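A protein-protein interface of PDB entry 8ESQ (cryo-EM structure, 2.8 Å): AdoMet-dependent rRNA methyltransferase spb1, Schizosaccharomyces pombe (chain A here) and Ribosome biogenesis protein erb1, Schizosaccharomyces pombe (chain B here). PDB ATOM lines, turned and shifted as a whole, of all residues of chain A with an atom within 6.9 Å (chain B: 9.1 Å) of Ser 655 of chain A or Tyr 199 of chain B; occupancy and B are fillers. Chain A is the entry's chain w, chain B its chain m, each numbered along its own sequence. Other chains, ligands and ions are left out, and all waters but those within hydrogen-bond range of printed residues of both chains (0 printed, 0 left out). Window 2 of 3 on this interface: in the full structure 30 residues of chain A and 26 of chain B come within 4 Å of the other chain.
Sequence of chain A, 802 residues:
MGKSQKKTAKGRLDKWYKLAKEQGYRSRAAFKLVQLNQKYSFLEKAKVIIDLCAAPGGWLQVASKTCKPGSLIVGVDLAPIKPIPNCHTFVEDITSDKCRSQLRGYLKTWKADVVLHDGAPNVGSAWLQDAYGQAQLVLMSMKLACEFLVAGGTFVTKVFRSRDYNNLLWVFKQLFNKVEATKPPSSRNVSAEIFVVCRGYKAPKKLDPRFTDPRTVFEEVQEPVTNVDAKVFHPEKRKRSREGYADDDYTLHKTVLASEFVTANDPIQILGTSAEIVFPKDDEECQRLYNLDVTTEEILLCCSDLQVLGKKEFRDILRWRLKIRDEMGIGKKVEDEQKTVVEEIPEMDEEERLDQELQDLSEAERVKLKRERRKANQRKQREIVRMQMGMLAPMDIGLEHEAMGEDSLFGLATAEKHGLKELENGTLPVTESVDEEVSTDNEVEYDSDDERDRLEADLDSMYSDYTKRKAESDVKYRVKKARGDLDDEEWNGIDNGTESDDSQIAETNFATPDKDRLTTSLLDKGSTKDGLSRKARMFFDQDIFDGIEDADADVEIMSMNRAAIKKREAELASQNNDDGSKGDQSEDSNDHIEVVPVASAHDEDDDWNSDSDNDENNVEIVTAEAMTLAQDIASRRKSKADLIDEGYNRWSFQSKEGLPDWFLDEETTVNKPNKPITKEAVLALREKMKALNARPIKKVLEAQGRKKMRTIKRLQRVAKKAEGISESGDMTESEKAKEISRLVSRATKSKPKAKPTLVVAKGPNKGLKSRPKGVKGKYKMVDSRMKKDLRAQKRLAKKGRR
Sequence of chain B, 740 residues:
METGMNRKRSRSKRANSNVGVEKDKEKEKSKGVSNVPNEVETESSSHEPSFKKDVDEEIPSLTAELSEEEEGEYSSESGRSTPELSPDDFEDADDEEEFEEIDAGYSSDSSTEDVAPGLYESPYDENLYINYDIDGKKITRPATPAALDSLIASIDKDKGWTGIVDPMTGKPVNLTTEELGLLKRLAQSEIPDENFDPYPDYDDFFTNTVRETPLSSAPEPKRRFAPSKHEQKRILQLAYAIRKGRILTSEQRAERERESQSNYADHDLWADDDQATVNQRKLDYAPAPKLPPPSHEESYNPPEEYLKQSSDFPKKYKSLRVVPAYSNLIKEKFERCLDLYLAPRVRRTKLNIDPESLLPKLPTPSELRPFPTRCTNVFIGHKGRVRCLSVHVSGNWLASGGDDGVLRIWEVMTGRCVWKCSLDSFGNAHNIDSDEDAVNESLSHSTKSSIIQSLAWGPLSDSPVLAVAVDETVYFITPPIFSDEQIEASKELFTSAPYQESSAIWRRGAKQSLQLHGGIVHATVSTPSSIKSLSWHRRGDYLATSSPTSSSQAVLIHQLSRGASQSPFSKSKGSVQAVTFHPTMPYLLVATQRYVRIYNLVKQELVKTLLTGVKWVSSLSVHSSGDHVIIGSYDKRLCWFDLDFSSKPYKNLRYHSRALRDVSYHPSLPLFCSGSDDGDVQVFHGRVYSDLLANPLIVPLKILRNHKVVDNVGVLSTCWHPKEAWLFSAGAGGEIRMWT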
ATOM      1  N   ARG A 650     -16.035 -14.718  -1.625  1.00  0.00           N
ATOM      2  CA  ARG A 650     -16.326 -13.685  -0.638  1.00  0.00           C
ATOM      3  C   ARG A 650     -15.631 -12.372  -0.966  1.00  0.00           C
ATOM      4  O   ARG A 650     -16.089 -11.306  -0.541  1.00  0.00           O
ATOM      5  CB  ARG A 650     -15.913 -14.162   0.756  1.00  0.00           C
ATOM      6  CG  ARG A 650     -14.416 -14.101   1.005  1.00  0.00           C
ATOM      7  CD  ARG A 650     -14.063 -14.356   2.454  1.00  0.00           C
ATOM      8  NE  ARG A 650     -14.215 -15.759   2.812  1.00  0.00           N
ATOM      9  CZ  ARG A 650     -14.787 -16.191   3.928  1.00  0.00           C
ATOM     10  NH1 ARG A 650     -15.245 -15.353   4.841  1.00  0.00           N
ATOM     11  NH2 ARG A 650     -14.897 -17.500   4.134  1.00  0.00           N
ATOM     12  N   TRP A 651     -14.530 -12.422  -1.713  1.00  0.00           N
ATOM     13  CA  TRP A 651     -13.728 -11.234  -1.962  1.00  0.00           C
ATOM     14  C   TRP A 651     -14.135 -10.497  -3.227  1.00  0.00           C
ATOM     15  O   TRP A 651     -14.002  -9.271  -3.286  1.00  0.00           O
ATOM     16  CB  TRP A 651     -12.249 -11.611  -2.036  1.00  0.00           C
ATOM     17  CG  TRP A 651     -11.624 -11.736  -0.690  1.00  0.00           C
ATOM     18  CD1 TRP A 651     -11.456 -10.745   0.232  1.00  0.00           C
ATOM     19  CD2 TRP A 651     -11.103 -12.927  -0.097  1.00  0.00           C
ATOM     20  NE1 TRP A 651     -10.851 -11.244   1.357  1.00  0.00           N
ATOM     21  CE2 TRP A 651     -10.626 -12.582   1.181  1.00  0.00           C
ATOM     22  CE3 TRP A 651     -10.990 -14.251  -0.526  1.00  0.00           C
ATOM     23  CZ2 TRP A 651     -10.044 -13.511   2.034  1.00  0.00           C
ATOM     24  CZ3 TRP A 651     -10.412 -15.171   0.322  1.00  0.00           C
ATOM     25  CH2 TRP A 651      -9.945 -14.797   1.589  1.00  0.00           C
ATOM     26  N   SER A 652     -14.623 -11.209  -4.241  1.00  0.00           N
ATOM     27  CA  SER A 652     -15.086 -10.538  -5.448  1.00  0.00           C
ATOM     28  C   SER A 652     -16.394  -9.798  -5.209  1.00  0.00           C
ATOM     29  O   SER A 652     -16.689  -8.822  -5.906  1.00  0.00           O
ATOM     30  CB  SER A 652     -15.245 -11.548  -6.581  1.00  0.00           C
ATOM     31  OG  SER A 652     -16.416 -12.323  -6.418  1.00  0.00           O
ATOM     32  N   PHE A 653     -17.183 -10.238  -4.234  1.00  0.00           N
ATOM     33  CA  PHE A 653     -18.424  -9.561  -3.891  1.00  0.00           C
ATOM     34  C   PHE A 653     -18.211  -8.380  -2.958  1.00  0.00           C
ATOM     35  O   PHE A 653     -19.178  -7.683  -2.633  1.00  0.00           O
ATOM     36  CB  PHE A 653     -19.407 -10.553  -3.271  1.00  0.00           C
ATOM     37  CG  PHE A 653     -20.269 -11.244  -4.279  1.00  0.00           C
ATOM     38  CD1 PHE A 653     -19.713 -12.096  -5.213  1.00  0.00           C
ATOM     39  CD2 PHE A 653     -21.631 -11.032  -4.303  1.00  0.00           C
ATOM     40  CE1 PHE A 653     -20.500 -12.730  -6.145  1.00  0.00           C
ATOM     41  CE2 PHE A 653     -22.422 -11.662  -5.233  1.00  0.00           C
ATOM     42  CZ  PHE A 653     -21.856 -12.511  -6.155  1.00  0.00           C
ATOM     43  N   GLN A 654     -16.975  -8.143  -2.523  1.00  0.00           N
ATOM     44  CA  GLN A 654     -16.613  -6.928  -1.798  1.00  0.00           C
ATOM     45  C   GLN A 654     -16.081  -5.927  -2.818  1.00  0.00           C
ATOM     46  O   GLN A 654     -14.878  -5.801  -3.054  1.00  0.00           O
ATOM     47  CB  GLN A 654     -15.589  -7.237  -0.717  1.00  0.00           C
ATOM     48  CG  GLN A 654     -16.138  -8.020   0.450  1.00  0.00           C
ATOM     49  CD  GLN A 654     -15.084  -8.292   1.488  1.00  0.00           C
ATOM     50  OE1 GLN A 654     -13.982  -7.754   1.421  1.00  0.00           O
ATOM     51  NE2 GLN A 654     -15.412  -9.131   2.459  1.00  0.00           N
ATOM     52  N   SER A 655     -17.008  -5.201  -3.434  1.00  0.00           N
ATOM     53  CA  SER A 655     -16.664  -4.329  -4.548  1.00  0.00           C
ATOM     54  C   SER A 655     -15.903  -3.097  -4.076  1.00  0.00           C
ATOM     55  O   SER A 655     -16.181  -2.544  -3.010  1.00  0.00           O
ATOM     56  CB  SER A 655     -17.926  -3.909  -5.294  1.00  0.00           C
ATOM     57  OG  SER A 655     -17.629  -2.994  -6.330  1.00  0.00           O
ATOM     58  N   LYS A 656     -14.940  -2.666  -4.887  1.00  0.00           N
ATOM     59  CA  LYS A 656     -14.104  -1.513  -4.587  1.00  0.00           C
ATOM     60  C   LYS A 656     -14.490  -0.276  -5.385  1.00  0.00           C
ATOM     61  O   LYS A 656     -13.717   0.684  -5.430  1.00  0.00           O
ATOM     62  CB  LYS A 656     -12.637  -1.853  -4.848  1.00  0.00           C
ATOM     63  CG  LYS A 656     -12.168  -3.104  -4.142  1.00  0.00           C
ATOM     64  CD  LYS A 656     -10.727  -3.421  -4.474  1.00  0.00           C
ATOM     65  CE  LYS A 656     -10.357  -4.800  -3.966  1.00  0.00           C
ATOM     66  NZ  LYS A 656     -11.154  -5.860  -4.640  1.00  0.00           N
ATOM     67  N   GLU A 657     -15.665  -0.273  -6.009  1.00  0.00           N
ATOM     68  CA  GLU A 657     -16.045   0.781  -6.947  1.00  0.00           C
ATOM     69  C   GLU A 657     -16.542   1.998  -6.180  1.00  0.00           C
ATOM     70  O   GLU A 657     -17.662   2.008  -5.666  1.00  0.00           O
ATOM     71  CB  GLU A 657     -17.106   0.276  -7.917  1.00  0.00           C
ATOM     72  CG  GLU A 657     -16.719  -0.998  -8.645  1.00  0.00           C
ATOM     73  CD  GLU A 657     -15.503  -0.823  -9.528  1.00  0.00           C
ATOM     74  OE1 GLU A 657     -15.359   0.258 -10.136  1.00  0.00           O
ATOM     75  OE2 GLU A 657     -14.689  -1.766  -9.611  1.00  0.00           O
ATOM     76  N   GLY A 658     -15.712   3.034  -6.112  1.00  0.00           N
ATOM     77  CA  GLY A 658     -16.097   4.295  -5.517  1.00  0.00           C
ATOM     78  C   GLY A 658     -15.653   4.515  -4.091  1.00  0.00           C
ATOM     79  O   GLY A 658     -16.040   5.523  -3.492  1.00  0.00           O
ATOM     80  N   LEU A 659     -14.868   3.618  -3.531  1.00  0.00           N
ATOM     81  CA  LEU A 659     -14.478   3.762  -2.141  1.00  0.00           C
ATOM     82  C   LEU A 659     -13.346   4.780  -2.004  1.00  0.00           C
ATOM     83  O   LEU A 659     -12.558   4.971  -2.933  1.00  0.00           O
ATOM     84  CB  LEU A 659     -14.044   2.417  -1.568  1.00  0.00           C
ATOM     85  CG  LEU A 659     -15.155   1.455  -1.133  1.00  0.00           C
ATOM     86  CD1 LEU A 659     -16.028   2.111  -0.079  1.00  0.00           C
ATOM     87  CD2 LEU A 659     -15.993   0.941  -2.287  1.00  0.00           C
ATOM     88  N   PHE A 663      -9.763   4.423   2.729  1.00  0.00           N
ATOM     89  CA  PHE A 663     -10.317   3.092   2.919  1.00  0.00           C
ATOM     90  C   PHE A 663      -9.676   2.073   1.984  1.00  0.00           C
ATOM     91  O   PHE A 663      -9.316   0.974   2.415  1.00  0.00           O
ATOM     92  CB  PHE A 663     -11.832   3.120   2.703  1.00  0.00           C
ATOM     93  CG  PHE A 663     -12.481   1.774   2.804  1.00  0.00           C
ATOM     94  CD1 PHE A 663     -12.471   1.072   3.997  1.00  0.00           C
ATOM     95  CD2 PHE A 663     -13.091   1.206   1.707  1.00  0.00           C
ATOM     96  CE1 PHE A 663     -13.068  -0.168   4.089  1.00  0.00           C
ATOM     97  CE2 PHE A 663     -13.691  -0.032   1.794  1.00  0.00           C
ATOM     98  CZ  PHE A 663     -13.679  -0.719   2.987  1.00  0.00           C
ATOM     99  N   LEU A 664      -9.522   2.428   0.708  1.00  0.00           N
ATOM    100  CA  LEU A 664      -8.998   1.484  -0.274  1.00  0.00           C
ATOM    101  C   LEU A 664      -7.548   1.117   0.009  1.00  0.00           C
ATOM    102  O   LEU A 664      -7.132  -0.016  -0.250  1.00  0.00           O
ATOM    103  CB  LEU A 664      -9.130   2.066  -1.679  1.00  0.00           C
ATOM    104  CG  LEU A 664     -10.469   1.859  -2.375  1.00  0.00           C
ATOM    105  CD1 LEU A 664     -10.345   2.191  -3.848  1.00  0.00           C
ATOM    106  CD2 LEU A 664     -10.949   0.433  -2.182  1.00  0.00           C
ATOM    107  N   ARG B 185      -9.847  -9.242 -14.290  1.00  0.00           N
ATOM    108  CA  ARG B 185     -10.905  -9.296 -13.287  1.00  0.00           C
ATOM    109  C   ARG B 185     -10.574 -10.299 -12.189  1.00  0.00           C
ATOM    110  O   ARG B 185     -10.713  -9.999 -10.999  1.00  0.00           O
ATOM    111  CB  ARG B 185     -12.237  -9.635 -13.950  1.00  0.00           C
ATOM    112  CG  ARG B 185     -12.585  -8.739 -15.121  1.00  0.00           C
ATOM    113  CD  ARG B 185     -14.040  -8.886 -15.504  1.00  0.00           C
ATOM    114  NE  ARG B 185     -14.927  -8.403 -14.454  1.00  0.00           N
ATOM    115  CZ  ARG B 185     -15.525  -7.220 -14.461  1.00  0.00           C
ATOM    116  NH1 ARG B 185     -15.361  -6.370 -15.462  1.00  0.00           N
ATOM    117  NH2 ARG B 185     -16.307  -6.882 -13.442  1.00  0.00           N
ATOM    118  N   GLN B 188      -7.698  -9.130  -9.895  1.00  0.00           N
ATOM    119  CA  GLN B 188      -8.067  -7.982  -9.081  1.00  0.00           C
ATOM    120  C   GLN B 188      -9.221  -8.284  -8.139  1.00  0.00           C
ATOM    121  O   GLN B 188      -9.682  -7.377  -7.439  1.00  0.00           O
ATOM    122  CB  GLN B 188      -8.424  -6.791  -9.972  1.00  0.00           C
ATOM    123  CG  GLN B 188      -7.230  -6.147 -10.647  1.00  0.00           C
ATOM    124  CD  GLN B 188      -7.532  -4.750 -11.146  1.00  0.00           C
ATOM    125  OE1 GLN B 188      -8.541  -4.521 -11.810  1.00  0.00           O
ATOM    126  NE2 GLN B 188      -6.658  -3.806 -10.824  1.00  0.00           N
ATOM    127  N   SER B 189      -9.693  -9.531  -8.111  1.00  0.00           N
ATOM    128  CA  SER B 189     -10.750  -9.981  -7.208  1.00  0.00           C
ATOM    129  C   SER B 189     -12.032  -9.172  -7.409  1.00  0.00           C
ATOM    130  O   SER B 189     -12.530  -8.500  -6.505  1.00  0.00           O
ATOM    131  CB  SER B 189     -10.286  -9.930  -5.749  1.00  0.00           C
ATOM    132  OG  SER B 189      -9.495 -11.060  -5.429  1.00  0.00           O
ATOM    133  N   GLU B 190     -12.558  -9.247  -8.626  1.00  0.00           N
ATOM    134  CA  GLU B 190     -13.879  -8.733  -8.942  1.00  0.00           C
ATOM    135  C   GLU B 190     -14.657  -9.819  -9.665  1.00  0.00           C
ATOM    136  O   GLU B 190     -14.126 -10.886  -9.979  1.00  0.00           O
ATOM    137  CB  GLU B 190     -13.818  -7.458  -9.789  1.00  0.00           C
ATOM    138  CG  GLU B 190     -12.740  -7.453 -10.842  1.00  0.00           C
ATOM    139  CD  GLU B 190     -12.171  -6.072 -11.075  1.00  0.00           C
ATOM    140  OE1 GLU B 190     -11.047  -5.969 -11.607  1.00  0.00           O
ATOM    141  OE2 GLU B 190     -12.848  -5.085 -10.721  1.00  0.00           O
ATOM    142  N   ILE B 191     -15.933  -9.544  -9.909  1.00  0.00           N
ATOM    143  CA  ILE B 191     -16.802 -10.502 -10.582  1.00  0.00           C
ATOM    144  C   ILE B 191     -16.237 -10.775 -11.969  1.00  0.00           C
ATOM    145  O   ILE B 191     -16.041  -9.836 -12.754  1.00  0.00           O
ATOM    146  CB  ILE B 191     -18.247  -9.993 -10.667  1.00  0.00           C
ATOM    147  CG1 ILE B 191     -18.694  -9.411  -9.326  1.00  0.00           C
ATOM    148  CG2 ILE B 191     -19.164 -11.115 -11.102  1.00  0.00           C
ATOM    149  CD1 ILE B 191     -18.684 -10.402  -8.199  1.00  0.00           C
ATOM    150  N   PHE B 196     -22.939  -8.827 -14.567  1.00  0.00           N
ATOM    151  CA  PHE B 196     -23.606  -9.632 -13.556  1.00  0.00           C
ATOM    152  C   PHE B 196     -23.992  -8.693 -12.430  1.00  0.00           C
ATOM    153  O   PHE B 196     -23.180  -7.863 -12.017  1.00  0.00           O
ATOM    154  CB  PHE B 196     -22.703 -10.749 -13.028  1.00  0.00           C
ATOM    155  CG  PHE B 196     -23.217 -11.398 -11.775  1.00  0.00           C
ATOM    156  CD1 PHE B 196     -24.378 -12.151 -11.794  1.00  0.00           C
ATOM    157  CD2 PHE B 196     -22.545 -11.247 -10.575  1.00  0.00           C
ATOM    158  CE1 PHE B 196     -24.852 -12.748 -10.642  1.00  0.00           C
ATOM    159  CE2 PHE B 196     -23.015 -11.839  -9.421  1.00  0.00           C
ATOM    160  CZ  PHE B 196     -24.170 -12.591  -9.455  1.00  0.00           C
ATOM    161  N   ASP B 197     -25.223  -8.809 -11.950  1.00  0.00           N
ATOM    162  CA  ASP B 197     -25.690  -7.896 -10.918  1.00  0.00           C
ATOM    163  C   ASP B 197     -25.276  -8.390  -9.539  1.00  0.00           C
ATOM    164  O   ASP B 197     -25.830  -9.379  -9.042  1.00  0.00           O
ATOM    165  CB  ASP B 197     -27.208  -7.737 -10.988  1.00  0.00           C
ATOM    166  CG  ASP B 197     -27.665  -6.361 -10.563  1.00  0.00           C
ATOM    167  OD1 ASP B 197     -26.828  -5.589 -10.050  1.00  0.00           O
ATOM    168  OD2 ASP B 197     -28.859  -6.048 -10.742  1.00  0.00           O
ATOM    169  N   PRO B 198     -24.317  -7.733  -8.883  1.00  0.00           N
ATOM    170  CA  PRO B 198     -23.990  -8.089  -7.503  1.00  0.00           C
ATOM    171  C   PRO B 198     -24.888  -7.410  -6.487  1.00  0.00           C
ATOM    172  O   PRO B 198     -24.739  -7.659  -5.285  1.00  0.00           O
ATOM    173  CB  PRO B 198     -22.543  -7.606  -7.370  1.00  0.00           C
ATOM    174  CG  PRO B 198     -22.496  -6.395  -8.249  1.00  0.00           C
ATOM    175  CD  PRO B 198     -23.537  -6.569  -9.338  1.00  0.00           C
ATOM    176  N   TYR B 199     -25.808  -6.566  -6.946  1.00  0.00           N
ATOM    177  CA  TYR B 199     -26.713  -5.819  -6.073  1.00  0.00           C
ATOM    178  C   TYR B 199     -28.146  -5.968  -6.565  1.00  0.00           C
ATOM    179  O   TYR B 199     -28.785  -4.988  -6.958  1.00  0.00           O
ATOM    180  CB  TYR B 199     -26.308  -4.350  -6.027  1.00  0.00           C
ATOM    181  CG  TYR B 199     -24.866  -4.135  -5.664  1.00  0.00           C
ATOM    182  CD1 TYR B 199     -24.344  -4.661  -4.497  1.00  0.00           C
ATOM    183  CD2 TYR B 199     -24.022  -3.412  -6.491  1.00  0.00           C
ATOM    184  CE1 TYR B 199     -23.030  -4.469  -4.158  1.00  0.00           C
ATOM    185  CE2 TYR B 199     -22.702  -3.216  -6.161  1.00  0.00           C
ATOM    186  CZ  TYR B 199     -22.213  -3.748  -4.992  1.00  0.00           C
ATOM    187  OH  TYR B 199     -20.899  -3.560  -4.646  1.00  0.00           O
ATOM    188  N   PRO B 200     -28.688  -7.183  -6.557  1.00  0.00           N
ATOM    189  CA  PRO B 200     -30.068  -7.363  -7.010  1.00  0.00           C
ATOM    190  C   PRO B 200     -31.048  -6.764  -6.016  1.00  0.00           C
ATOM    191  O   PRO B 200     -30.771  -6.661  -4.819  1.00  0.00           O
ATOM    192  CB  PRO B 200     -30.218  -8.883  -7.096  1.00  0.00           C
ATOM    193  CG  PRO B 200     -29.263  -9.398  -6.099  1.00  0.00           C
ATOM    194  CD  PRO B 200     -28.110  -8.441  -6.053  1.00  0.00           C
ATOM    195  N   ASP B 201     -32.206  -6.363  -6.527  1.00  0.00           N
ATOM    196  CA  ASP B 201     -33.226  -5.784  -5.670  1.00  0.00           C
ATOM    197  C   ASP B 201     -33.732  -6.819  -4.678  1.00  0.00           C
ATOM    198  O   ASP B 201     -33.679  -8.026  -4.925  1.00  0.00           O
ATOM    199  CB  ASP B 201     -34.383  -5.240  -6.502  1.00  0.00           C
ATOM    200  CG  ASP B 201     -34.133  -3.831  -6.982  1.00  0.00           C
ATOM    201  OD1 ASP B 201     -33.382  -3.101  -6.303  1.00  0.00           O
ATOM    202  OD2 ASP B 201     -34.682  -3.451  -8.036  1.00  0.00           O
ATOM    203  N   TYR B 202     -34.209  -6.333  -3.535  1.00  0.00           N
ATOM    204  CA  TYR B 202     -34.645  -7.226  -2.473  1.00  0.00           C
ATOM    205  C   TYR B 202     -35.773  -8.120  -2.961  1.00  0.00           C
ATOM    206  O   TYR B 202     -36.734  -7.653  -3.577  1.00  0.00           O
ATOM    207  CB  TYR B 202     -35.092  -6.422  -1.257  1.00  0.00           C
ATOM    208  CG  TYR B 202     -35.707  -7.255  -0.160  1.00  0.00           C
ATOM    209  CD1 TYR B 202     -34.914  -7.986   0.711  1.00  0.00           C
ATOM    210  CD2 TYR B 202     -37.082  -7.302   0.010  1.00  0.00           C
ATOM    211  CE1 TYR B 202     -35.472  -8.743   1.713  1.00  0.00           C
ATOM    212  CE2 TYR B 202     -37.647  -8.056   1.009  1.00  0.00           C
ATOM    213  CZ  TYR B 202     -36.839  -8.775   1.856  1.00  0.00           C
ATOM    214  OH  TYR B 202     -37.406  -9.523   2.857  1.00  0.00           O
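O of Arg 185 of chain B sits at hydrogen-bond distance from N of Glu 190 of chain B, at 3.1 Å. NE of Arg 185 of chain B lies within hydrogen-bond range of O of Ile 191 of chain B, at 2.5 Å. OE1 of Gln 188 of chain B lies close to OE1 of Glu 190 of chain B, 2.9 Å away. OD1 of Asp 197 of chain B lies close to N of Tyr 199 of chain B, at 3.4 Å. The backbone NH (N) of Glu 657 of chain A sits close to the side-chain hydroxyl (OG) of Ser 655 of chain A, 3.4 Å away.
Ser 189 of chain B touches Trp 651 of chain A (O to O, 3.6 Å). Ser 652 of chain A touches Ser 189 of chain B (CA to O, 3.4 Å). Ser 652 of chain A touches Glu 190 of chain B. Ile 191 of chain B touches Ser 652 of chain A. Phe 653 of chain A touches Ile 191 of chain B (CD1 to CD1, 3.6 Å). Phe 653 of chain A touches Phe 196 of chain B (CZ to CE2, 3.5 Å). Ser 655 of chain A touches Tyr 199 of chain B. Gln 188 of chain B touches Lys 656 of chain A. Lys 656 of chain A touches Ser 189 of chain B. Glu 657 of chain A touches Glu 190 of chain B.
Ser 655 of chain A touches one residue of chain B. Of chain A, only Ser 655 (3.1 Å) comes within 4 Å of Tyr 199 of chain B. Of the printed residues of chain A, Ser 189 of chain B touches Trp 651, Ser 652 and Lys 656. Of the printed residues of chain A, Ile 191 of chain B touches Ser 652 (3.4 Å) and Phe 653 (3.6 Å). Of the printed residues of chain A, Phe 196 of chain B touches Phe 653 (3.5 Å). The nearest residue of chain B that does not touch Ser 655 of chain A is Pro 198 of chain B (6.0 Å).
Of the 12 printed residues of chain A, 6 touch a printed residue of chain B. Hydrophobic or aromatic side chains of chain A within 4 Å of the printed part of chain B: Phe 653. Hydrophobic or aromatic side chains of chain B that line the printed part of chain A: Ile 191, Phe 196 and Tyr 199. Among the printed residues, no Asp or Glu carboxylate lies within 4 Å of a Lys or Arg side-chain nitrogen of the other chain.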
